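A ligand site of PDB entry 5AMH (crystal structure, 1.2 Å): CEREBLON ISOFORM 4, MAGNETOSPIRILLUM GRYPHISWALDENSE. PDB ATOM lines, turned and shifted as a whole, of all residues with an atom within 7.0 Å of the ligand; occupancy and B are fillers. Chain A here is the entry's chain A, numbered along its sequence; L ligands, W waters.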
ATOM      1  N   VAL A  49      27.791  24.631  20.589  1.00  0.00           N
ATOM      2  CA  VAL A  49      26.493  24.199  20.194  1.00  0.00           C
ATOM      3  C   VAL A  49      25.429  24.811  21.128  1.00  0.00           C
ATOM      4  O   VAL A  49      25.739  25.226  22.236  1.00  0.00           O
ATOM      5  CB  VAL A  49      26.363  22.655  20.198  1.00  0.00           C
ATOM      6  CG1 VAL A  49      27.421  22.007  19.333  1.00  0.00           C
ATOM      7  CG2 VAL A  49      26.417  22.126  21.635  1.00  0.00           C
ATOM      8  N   PHE A  50      24.214  24.852  20.605  1.00  0.00           N
ATOM      9  CA  PHE A  50      23.036  25.331  21.367  1.00  0.00           C
ATOM     10  C   PHE A  50      22.033  24.205  21.503  1.00  0.00           C
ATOM     11  O   PHE A  50      21.687  23.570  20.527  1.00  0.00           O
ATOM     12  CB  PHE A  50      22.299  26.463  20.597  1.00  0.00           C
ATOM     13  CG  PHE A  50      23.045  27.720  20.511  1.00  0.00           C
ATOM     14  CD1 PHE A  50      24.070  27.883  19.586  1.00  0.00           C
ATOM     15  CD2 PHE A  50      22.650  28.811  21.306  1.00  0.00           C
ATOM     16  CE1 PHE A  50      24.769  29.096  19.526  1.00  0.00           C
ATOM     17  CE2 PHE A  50      23.324  30.037  21.238  1.00  0.00           C
ATOM     18  CZ  PHE A  50      24.352  30.160  20.358  1.00  0.00           C
ATOM     19  N   ASN A  51      21.539  24.043  22.742  1.00  0.00           N
ATOM     20  CA  ASN A  51      20.441  23.123  22.933  1.00  0.00           C
ATOM     21  C   ASN A  51      19.129  23.848  22.605  1.00  0.00           C
ATOM     22  O   ASN A  51      19.107  25.024  22.337  1.00  0.00           O
ATOM     23  CB  ASN A  51      20.500  22.469  24.308  1.00  0.00           C
ATOM     24  CG  ASN A  51      20.015  23.343  25.419  1.00  0.00           C
ATOM     25  OD1 ASN A  51      19.534  24.450  25.237  1.00  0.00           O
ATOM     26  ND2 ASN A  51      20.046  22.770  26.650  1.00  0.00           N
ATOM     27  N   PRO A  52      18.005  23.085  22.597  1.00  0.00           N
ATOM     28  CA  PRO A  52      16.758  23.739  22.175  1.00  0.00           C
ATOM     29  C   PRO A  52      16.269  24.791  23.150  1.00  0.00           C
ATOM     30  O   PRO A  52      15.388  25.579  22.753  1.00  0.00           O
ATOM     31  CB  PRO A  52      15.755  22.543  22.115  1.00  0.00           C
ATOM     32  CG  PRO A  52      16.641  21.326  21.733  1.00  0.00           C
ATOM     33  CD  PRO A  52      17.891  21.621  22.564  1.00  0.00           C
ATOM     34  N   ALA A  53      16.751  24.842  24.386  1.00  0.00           N
ATOM     35  CA  ALA A  53      16.408  25.898  25.339  1.00  0.00           C
ATOM     36  C   ALA A  53      17.273  27.103  25.119  1.00  0.00           C
ATOM     37  O   ALA A  53      17.115  28.114  25.805  1.00  0.00           O
ATOM     38  CB  ALA A  53      16.596  25.387  26.727  1.00  0.00           C
ATOM     39  N   PHE A  57      26.703  25.053  24.907  1.00  0.00           N
ATOM     40  CA  PHE A  57      27.668  24.087  25.432  1.00  0.00           C
ATOM     41  C   PHE A  57      28.936  24.111  24.572  1.00  0.00           C
ATOM     42  O   PHE A  57      28.816  24.289  23.345  1.00  0.00           O
ATOM     43  CB  PHE A  57      27.156  22.627  25.427  1.00  0.00           C
ATOM     44  CG  PHE A  57      25.898  22.411  26.226  1.00  0.00           C
ATOM     45  CD1 PHE A  57      25.836  22.647  27.593  1.00  0.00           C
ATOM     46  CD2 PHE A  57      24.865  21.746  25.654  1.00  0.00           C
ATOM     47  CE1 PHE A  57      24.676  22.398  28.330  1.00  0.00           C
ATOM     48  CE2 PHE A  57      23.695  21.460  26.354  1.00  0.00           C
ATOM     49  CZ  PHE A  57      23.616  21.806  27.679  1.00  0.00           C
ATOM     50  N   SER A  75      18.458   8.820  18.826  1.00  0.00           N
ATOM     51  CA  SER A  75      17.640   9.789  18.185  1.00  0.00           C
ATOM     52  C   SER A  75      18.463  10.653  17.280  1.00  0.00           C
ATOM     53  O   SER A  75      19.584  11.014  17.604  1.00  0.00           O
ATOM     54  CB  SER A  75      16.971  10.746  19.215  1.00  0.00           C
ATOM     55  OG  SER A  75      16.181  11.675  18.464  1.00  0.00           O
ATOM     56  N   GLY A  76      17.894  11.016  16.140  1.00  0.00           N
ATOM     57  CA  GLY A  76      18.528  11.923  15.245  1.00  0.00           C
ATOM     58  C   GLY A  76      18.098  13.358  15.402  1.00  0.00           C
ATOM     59  O   GLY A  76      18.759  14.282  14.908  1.00  0.00           O
ATOM     60  N   GLU A  77      17.072  13.603  16.214  1.00  0.00           N
ATOM     61  CA  GLU A  77      16.525  14.963  16.264  1.00  0.00           C
ATOM     62  C   GLU A  77      17.498  15.894  16.916  1.00  0.00           C
ATOM     63  O   GLU A  77      18.134  15.588  17.919  1.00  0.00           O
ATOM     64  CB  GLU A  77      15.245  14.962  17.033  1.00  0.00           C
ATOM     65  CG  GLU A  77      14.016  14.723  16.226  1.00  0.00           C
ATOM     66  CD  GLU A  77      12.842  15.155  17.058  1.00  0.00           C
ATOM     67  OE1 GLU A  77      12.716  14.627  18.173  1.00  0.00           O
ATOM     68  OE2 GLU A  77      12.113  16.086  16.652  1.00  0.00           O
ATOM     69  N   PHE A  78      17.629  17.066  16.330  1.00  0.00           N
ATOM     70  CA  PHE A  78      18.467  18.116  16.864  1.00  0.00           C
ATOM     71  C   PHE A  78      20.001  17.772  16.864  1.00  0.00           C
ATOM     72  O   PHE A  78      20.785  18.514  17.412  1.00  0.00           O
ATOM     73  CB  PHE A  78      18.061  18.527  18.278  1.00  0.00           C
ATOM     74  CG  PHE A  78      16.661  18.992  18.370  1.00  0.00           C
ATOM     75  CD1 PHE A  78      16.278  20.116  17.714  1.00  0.00           C
ATOM     76  CD2 PHE A  78      15.756  18.254  19.061  1.00  0.00           C
ATOM     77  CE1 PHE A  78      14.976  20.546  17.785  1.00  0.00           C
ATOM     78  CE2 PHE A  78      14.447  18.705  19.187  1.00  0.00           C
ATOM     79  CZ  PHE A  78      14.065  19.798  18.512  1.00  0.00           C
ATOM     80  N   SER A  79      20.373  16.648  16.206  1.00  0.00           N
ATOM     81  CA  SER A  79      21.788  16.279  16.302  1.00  0.00           C
ATOM     82  C   SER A  79      22.700  17.381  15.822  1.00  0.00           C
ATOM     83  O   SER A  79      22.477  17.899  14.722  1.00  0.00           O
ATOM     84  CB  SER A  79      22.036  15.002  15.544  1.00  0.00           C
ATOM     85  OG  SER A  79      23.395  14.674  15.686  1.00  0.00           O
ATOM     86  N   TRP A  80      23.739  17.644  16.589  1.00  0.00           N
ATOM     87  CA  TRP A  80      24.695  18.663  16.202  1.00  0.00           C
ATOM     88  C   TRP A  80      25.737  18.158  15.180  1.00  0.00           C
ATOM     89  O   TRP A  80      26.535  18.959  14.693  1.00  0.00           O
ATOM     90  CB  TRP A  80      25.429  19.182  17.422  1.00  0.00           C
ATOM     91  CG  TRP A  80      24.569  19.849  18.417  1.00  0.00           C
ATOM     92  CD1 TRP A  80      23.709  20.897  18.190  1.00  0.00           C
ATOM     93  CD2 TRP A  80      24.488  19.593  19.812  1.00  0.00           C
ATOM     94  NE1 TRP A  80      23.090  21.272  19.326  1.00  0.00           N
ATOM     95  CE2 TRP A  80      23.562  20.498  20.348  1.00  0.00           C
ATOM     96  CE3 TRP A  80      25.128  18.701  20.675  1.00  0.00           C
ATOM     97  CZ2 TRP A  80      23.253  20.512  21.711  1.00  0.00           C
ATOM     98  CZ3 TRP A  80      24.792  18.679  21.976  1.00  0.00           C
ATOM     99  CH2 TRP A  80      23.867  19.582  22.495  1.00  0.00           C
ATOM    100  N   PHE A  81      25.675  16.836  14.925  1.00  0.00           N
ATOM    101  CA  PHE A  81      26.707  16.201  14.051  1.00  0.00           C
ATOM    102  C   PHE A  81      25.941  15.447  12.977  1.00  0.00           C
ATOM    103  O   PHE A  81      25.268  14.449  13.200  1.00  0.00           O
ATOM    104  CB  PHE A  81      27.604  15.307  14.914  1.00  0.00           C
ATOM    105  CG  PHE A  81      28.302  16.014  16.001  1.00  0.00           C
ATOM    106  CD1 PHE A  81      29.531  16.652  15.754  1.00  0.00           C
ATOM    107  CD2 PHE A  81      27.788  16.031  17.291  1.00  0.00           C
ATOM    108  CE1 PHE A  81      30.179  17.250  16.799  1.00  0.00           C
ATOM    109  CE2 PHE A  81      28.457  16.687  18.301  1.00  0.00           C
ATOM    110  CZ  PHE A  81      29.649  17.299  18.067  1.00  0.00           C
ATOM    111  N   TYR A  84      24.739  11.611  12.402  1.00  0.00           N
ATOM    112  CA  TYR A  84      24.870  10.812  13.616  1.00  0.00           C
ATOM    113  C   TYR A  84      23.587  10.946  14.486  1.00  0.00           C
ATOM    114  O   TYR A  84      23.015  12.052  14.568  1.00  0.00           O
ATOM    115  CB  TYR A  84      26.040  11.230  14.511  1.00  0.00           C
ATOM    116  CG  TYR A  84      27.390  10.971  13.907  1.00  0.00           C
ATOM    117  CD1 TYR A  84      27.971  11.910  13.047  1.00  0.00           C
ATOM    118  CD2 TYR A  84      28.104   9.814  14.209  1.00  0.00           C
ATOM    119  CE1 TYR A  84      29.240  11.676  12.477  1.00  0.00           C
ATOM    120  CE2 TYR A  84      29.371   9.559  13.647  1.00  0.00           C
ATOM    121  CZ  TYR A  84      29.944  10.501  12.792  1.00  0.00           C
ATOM    122  OH  TYR A  84      31.159  10.306  12.175  1.00  0.00           O
ATOM    123  N   ASP A  85      23.195   9.820  15.061  1.00  0.00           N
ATOM    124  CA  ASP A  85      22.165   9.801  16.099  1.00  0.00           C
ATOM    125  C   ASP A  85      22.811   9.705  17.475  1.00  0.00           C
ATOM    126  O   ASP A  85      23.944   9.289  17.616  1.00  0.00           O
ATOM    127  CB  ASP A  85      21.317   8.527  15.955  1.00  0.00           C
ATOM    128  CG  ASP A  85      20.449   8.495  14.700  1.00  0.00           C
ATOM    129  OD1 ASP A  85      20.295   9.477  14.035  1.00  0.00           O
ATOM    130  OD2 ASP A  85      19.984   7.406  14.407  1.00  0.00           O
ATOM    131  N   TRP A  86      22.142  10.294  18.480  1.00  0.00           N
ATOM    132  CA  TRP A  86      22.673  10.401  19.823  1.00  0.00           C
ATOM    133  C   TRP A  86      21.871   9.563  20.826  1.00  0.00           C
ATOM    134  O   TRP A  86      20.664   9.373  20.665  1.00  0.00           O
ATOM    135  CB  TRP A  86      22.731  11.861  20.273  1.00  0.00           C
ATOM    136  CG  TRP A  86      21.476  12.607  20.178  1.00  0.00           C
ATOM    137  CD1 TRP A  86      21.075  13.337  19.116  1.00  0.00           C
ATOM    138  CD2 TRP A  86      20.423  12.651  21.109  1.00  0.00           C
ATOM    139  NE1 TRP A  86      19.839  13.895  19.321  1.00  0.00           N
ATOM    140  CE2 TRP A  86      19.399  13.459  20.535  1.00  0.00           C
ATOM    141  CE3 TRP A  86      20.203  12.083  22.387  1.00  0.00           C
ATOM    142  CZ2 TRP A  86      18.221  13.734  21.168  1.00  0.00           C
ATOM    143  CZ3 TRP A  86      19.054  12.409  23.022  1.00  0.00           C
ATOM    144  CH2 TRP A  86      18.045  13.193  22.387  1.00  0.00           C
ATOM    145  N   THR A  87      22.607   9.208  21.896  1.00  0.00           N
ATOM    146  CA  THR A  87      21.998   8.722  23.119  1.00  0.00           C
ATOM    147  C   THR A  87      22.655   9.444  24.250  1.00  0.00           C
ATOM    148  O   THR A  87      23.810   9.834  24.207  1.00  0.00           O
ATOM    149  CB  THR A  87      22.181   7.209  23.308  1.00  0.00           C
ATOM    150  OG1 THR A  87      23.571   6.882  23.248  1.00  0.00           O
ATOM    151  CG2 THR A  87      21.405   6.435  22.230  1.00  0.00           C
ATOM    152  N   ILE A  88      21.935   9.657  25.329  1.00  0.00           N
ATOM    153  CA  ILE A  88      22.422  10.383  26.499  1.00  0.00           C
ATOM    154  C   ILE A  88      23.440   9.558  27.266  1.00  0.00           C
ATOM    155  O   ILE A  88      23.219   8.357  27.531  1.00  0.00           O
ATOM    156  CB  ILE A  88      21.210  10.739  27.348  1.00  0.00           C
ATOM    157  CG1 ILE A  88      20.437  11.891  26.684  1.00  0.00           C
ATOM    158  CG2 ILE A  88      21.607  11.139  28.776  1.00  0.00           C
ATOM    159  CD1 ILE A  88      19.018  12.061  27.167  1.00  0.00           C
ATOM    160  N   HIS A  97      24.893  14.027  34.026  1.00  0.00           N
ATOM    161  CA  HIS A  97      24.766  14.027  32.608  1.00  0.00           C
ATOM    162  C   HIS A  97      25.972  14.661  31.960  1.00  0.00           C
ATOM    163  O   HIS A  97      26.138  15.863  31.936  1.00  0.00           O
ATOM    164  CB  HIS A  97      23.466  14.739  32.189  1.00  0.00           C
ATOM    165  CG  HIS A  97      23.244  14.716  30.729  1.00  0.00           C
ATOM    166  ND1 HIS A  97      22.361  15.549  30.112  1.00  0.00           N
ATOM    167  CD2 HIS A  97      23.860  14.026  29.749  1.00  0.00           C
ATOM    168  CE1 HIS A  97      22.405  15.380  28.778  1.00  0.00           C
ATOM    169  NE2 HIS A  97      23.336  14.468  28.563  1.00  0.00           N
ATOM    170  N   GLY A  99      27.200  14.053  28.691  1.00  0.00           N
ATOM    171  CA  GLY A  99      27.081  14.395  27.265  1.00  0.00           C
ATOM    172  C   GLY A  99      26.305  13.311  26.557  1.00  0.00           C
ATOM    173  O   GLY A  99      25.234  12.918  27.023  1.00  0.00           O
ATOM    174  N   TRP A 100      26.834  12.892  25.399  1.00  0.00           N
ATOM    175  CA  TRP A 100      26.112  12.025  24.490  1.00  0.00           C
ATOM    176  C   TRP A 100      27.085  11.093  23.791  1.00  0.00           C
ATOM    177  O   TRP A 100      28.249  11.429  23.597  1.00  0.00           O
ATOM    178  CB  TRP A 100      25.354  12.855  23.414  1.00  0.00           C
ATOM    179  CG  TRP A 100      24.425  13.793  23.987  1.00  0.00           C
ATOM    180  CD1 TRP A 100      23.132  13.646  24.347  1.00  0.00           C
ATOM    181  CD2 TRP A 100      24.765  15.135  24.438  1.00  0.00           C
ATOM    182  NE1 TRP A 100      22.642  14.719  25.000  1.00  0.00           N
ATOM    183  CE2 TRP A 100      23.623  15.676  25.033  1.00  0.00           C
ATOM    184  CE3 TRP A 100      25.902  15.908  24.364  1.00  0.00           C
ATOM    185  CZ2 TRP A 100      23.619  16.985  25.578  1.00  0.00           C
ATOM    186  CZ3 TRP A 100      25.879  17.155  24.892  1.00  0.00           C
ATOM    187  CH2 TRP A 100      24.754  17.685  25.500  1.00  0.00           C
ATOM    188  N   TYR A 102      27.381   9.235  20.098  1.00  0.00           N
ATOM    189  CA  TYR A 102      26.951   9.372  18.751  1.00  0.00           C
ATOM    190  C   TYR A 102      27.264   8.099  17.978  1.00  0.00           C
ATOM    191  O   TYR A 102      28.324   7.525  18.104  1.00  0.00           O
ATOM    192  CB  TYR A 102      27.608  10.606  18.112  1.00  0.00           C
ATOM    193  CG  TYR A 102      27.107  11.880  18.685  1.00  0.00           C
ATOM    194  CD1 TYR A 102      25.963  12.512  18.165  1.00  0.00           C
ATOM    195  CD2 TYR A 102      27.761  12.485  19.736  1.00  0.00           C
ATOM    196  CE1 TYR A 102      25.464  13.647  18.753  1.00  0.00           C
ATOM    197  CE2 TYR A 102      27.266  13.660  20.290  1.00  0.00           C
ATOM    198  CZ  TYR A 102      26.110  14.225  19.806  1.00  0.00           C
ATOM    199  OH  TYR A 102      25.677  15.414  20.374  1.00  0.00           O
HETATM  200  O1  LIG L   1      20.187  19.306  20.805  1.00  0.00           O
HETATM  201  C1  LIG L   1      20.819  18.263  20.998  1.00  0.00           C
HETATM  202  N1  LIG L   1      21.689  17.769  20.066  1.00  0.00           N
HETATM  203  C2  LIG L   1      22.498  16.670  20.238  1.00  0.00           C
HETATM  204  O2  LIG L   1      23.269  16.396  19.348  1.00  0.00           O
HETATM  205  C3  LIG L   1      22.403  15.915  21.518  1.00  0.00           C
HETATM  206  C4  LIG L   1      21.063  16.102  22.253  1.00  0.00           C
HETATM  207  C5  LIG L   1      20.767  17.561  22.338  1.00  0.00           C
HETATM  208  N2  LIG L   1      19.529  17.812  23.006  1.00  0.00           N
HETATM  209  C6  LIG L   1      16.116  19.565  25.497  1.00  0.00           C
HETATM  210  C7  LIG L   1      17.467  19.563  25.499  1.00  0.00           C
HETATM  211  C8  LIG L   1      18.020  18.785  24.427  1.00  0.00           C
HETATM  212  C9  LIG L   1      17.331  18.039  23.489  1.00  0.00           C
HETATM  213  O3  LIG L   1      20.428  19.219  24.673  1.00  0.00           O
HETATM  214  O4  LIG L   1      18.148  16.812  21.437  1.00  0.00           O
HETATM  215  C10 LIG L   1      15.904  18.046  23.559  1.00  0.00           C
HETATM  216  C11 LIG L   1      15.260  18.776  24.650  1.00  0.00           C
HETATM  217  C12 LIG L   1      18.310  17.524  22.490  1.00  0.00           C
HETATM  218  C13 LIG L   1      19.418  18.681  24.186  1.00  0.00           C
HETATM  219  O   HOH W   1      20.613  19.982  27.301  1.00  0.00           O
HETATM  220  O   HOH W   2      19.418  22.193  19.628  1.00  0.00           O
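The backbone carbonyl oxygen of Phe 50 lies within hydrogen-bond range of the indole nitrogen of Trp 80 (2.9 Å).
NE1 of Trp 86 lies within hydrogen-bond range of O of Glu 77, at 2.8 Å.
The backbone NH (N) of Trp 86 sits at hydrogen-bond distance from the backbone carbonyl oxygen (O) of Ser 75, at 2.8 Å.
OD1 of Asn 51 is in hydrogen-bond range of N of Ala 53 (2.9 Å).
The backbone carbonyl oxygen (O) of Phe 81 lies within hydrogen-bond range of the side-chain hydroxyl (OG) of Ser 79 (3.1 Å).
O of Tyr 84 sits at hydrogen-bond distance from OG of Ser 79.
N of Glu 77 lies within hydrogen-bond range of OG of Ser 75 (3.1 Å).
Water W1 lies within hydrogen-bond range of O3 of the ligand and ND2 of Asn 51.
Water W2 bridges O of Phe 50 and O1 of the ligand.
An oxygen (O2) of the ligand sits at hydrogen-bond distance from the side-chain hydroxyl (OH) of Tyr 102, at 2.8 Å.
The backbone carbonyl oxygen of Phe 78 is in hydrogen-bond range of a nitrogen (N1) of the ligand, at 2.9 Å.
The backbone NH of Trp 80 is in hydrogen-bond range of an oxygen (O2) of the ligand (3.1 Å).
Asn 51 touches the ligand.
Pro 52 touches the ligand.
O of Glu 77 touches O4 of the ligand, at 3.7 Å.
CA of Ser 79 touches O2 of the ligand (3.4 Å).
Trp 86 touches the ligand (CZ2 to O4, 3.1 Å).
NE1 of Trp 100 touches C4 of the ligand (3.5 Å).
Hydrophobic or aromatic side chains that line the ligand: Pro 52, Phe 78, Trp 80, Trp 86, Trp 100 and Tyr 102.
The nearest printed residue that does not touch the ligand is Phe 57 (4.3 Å).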
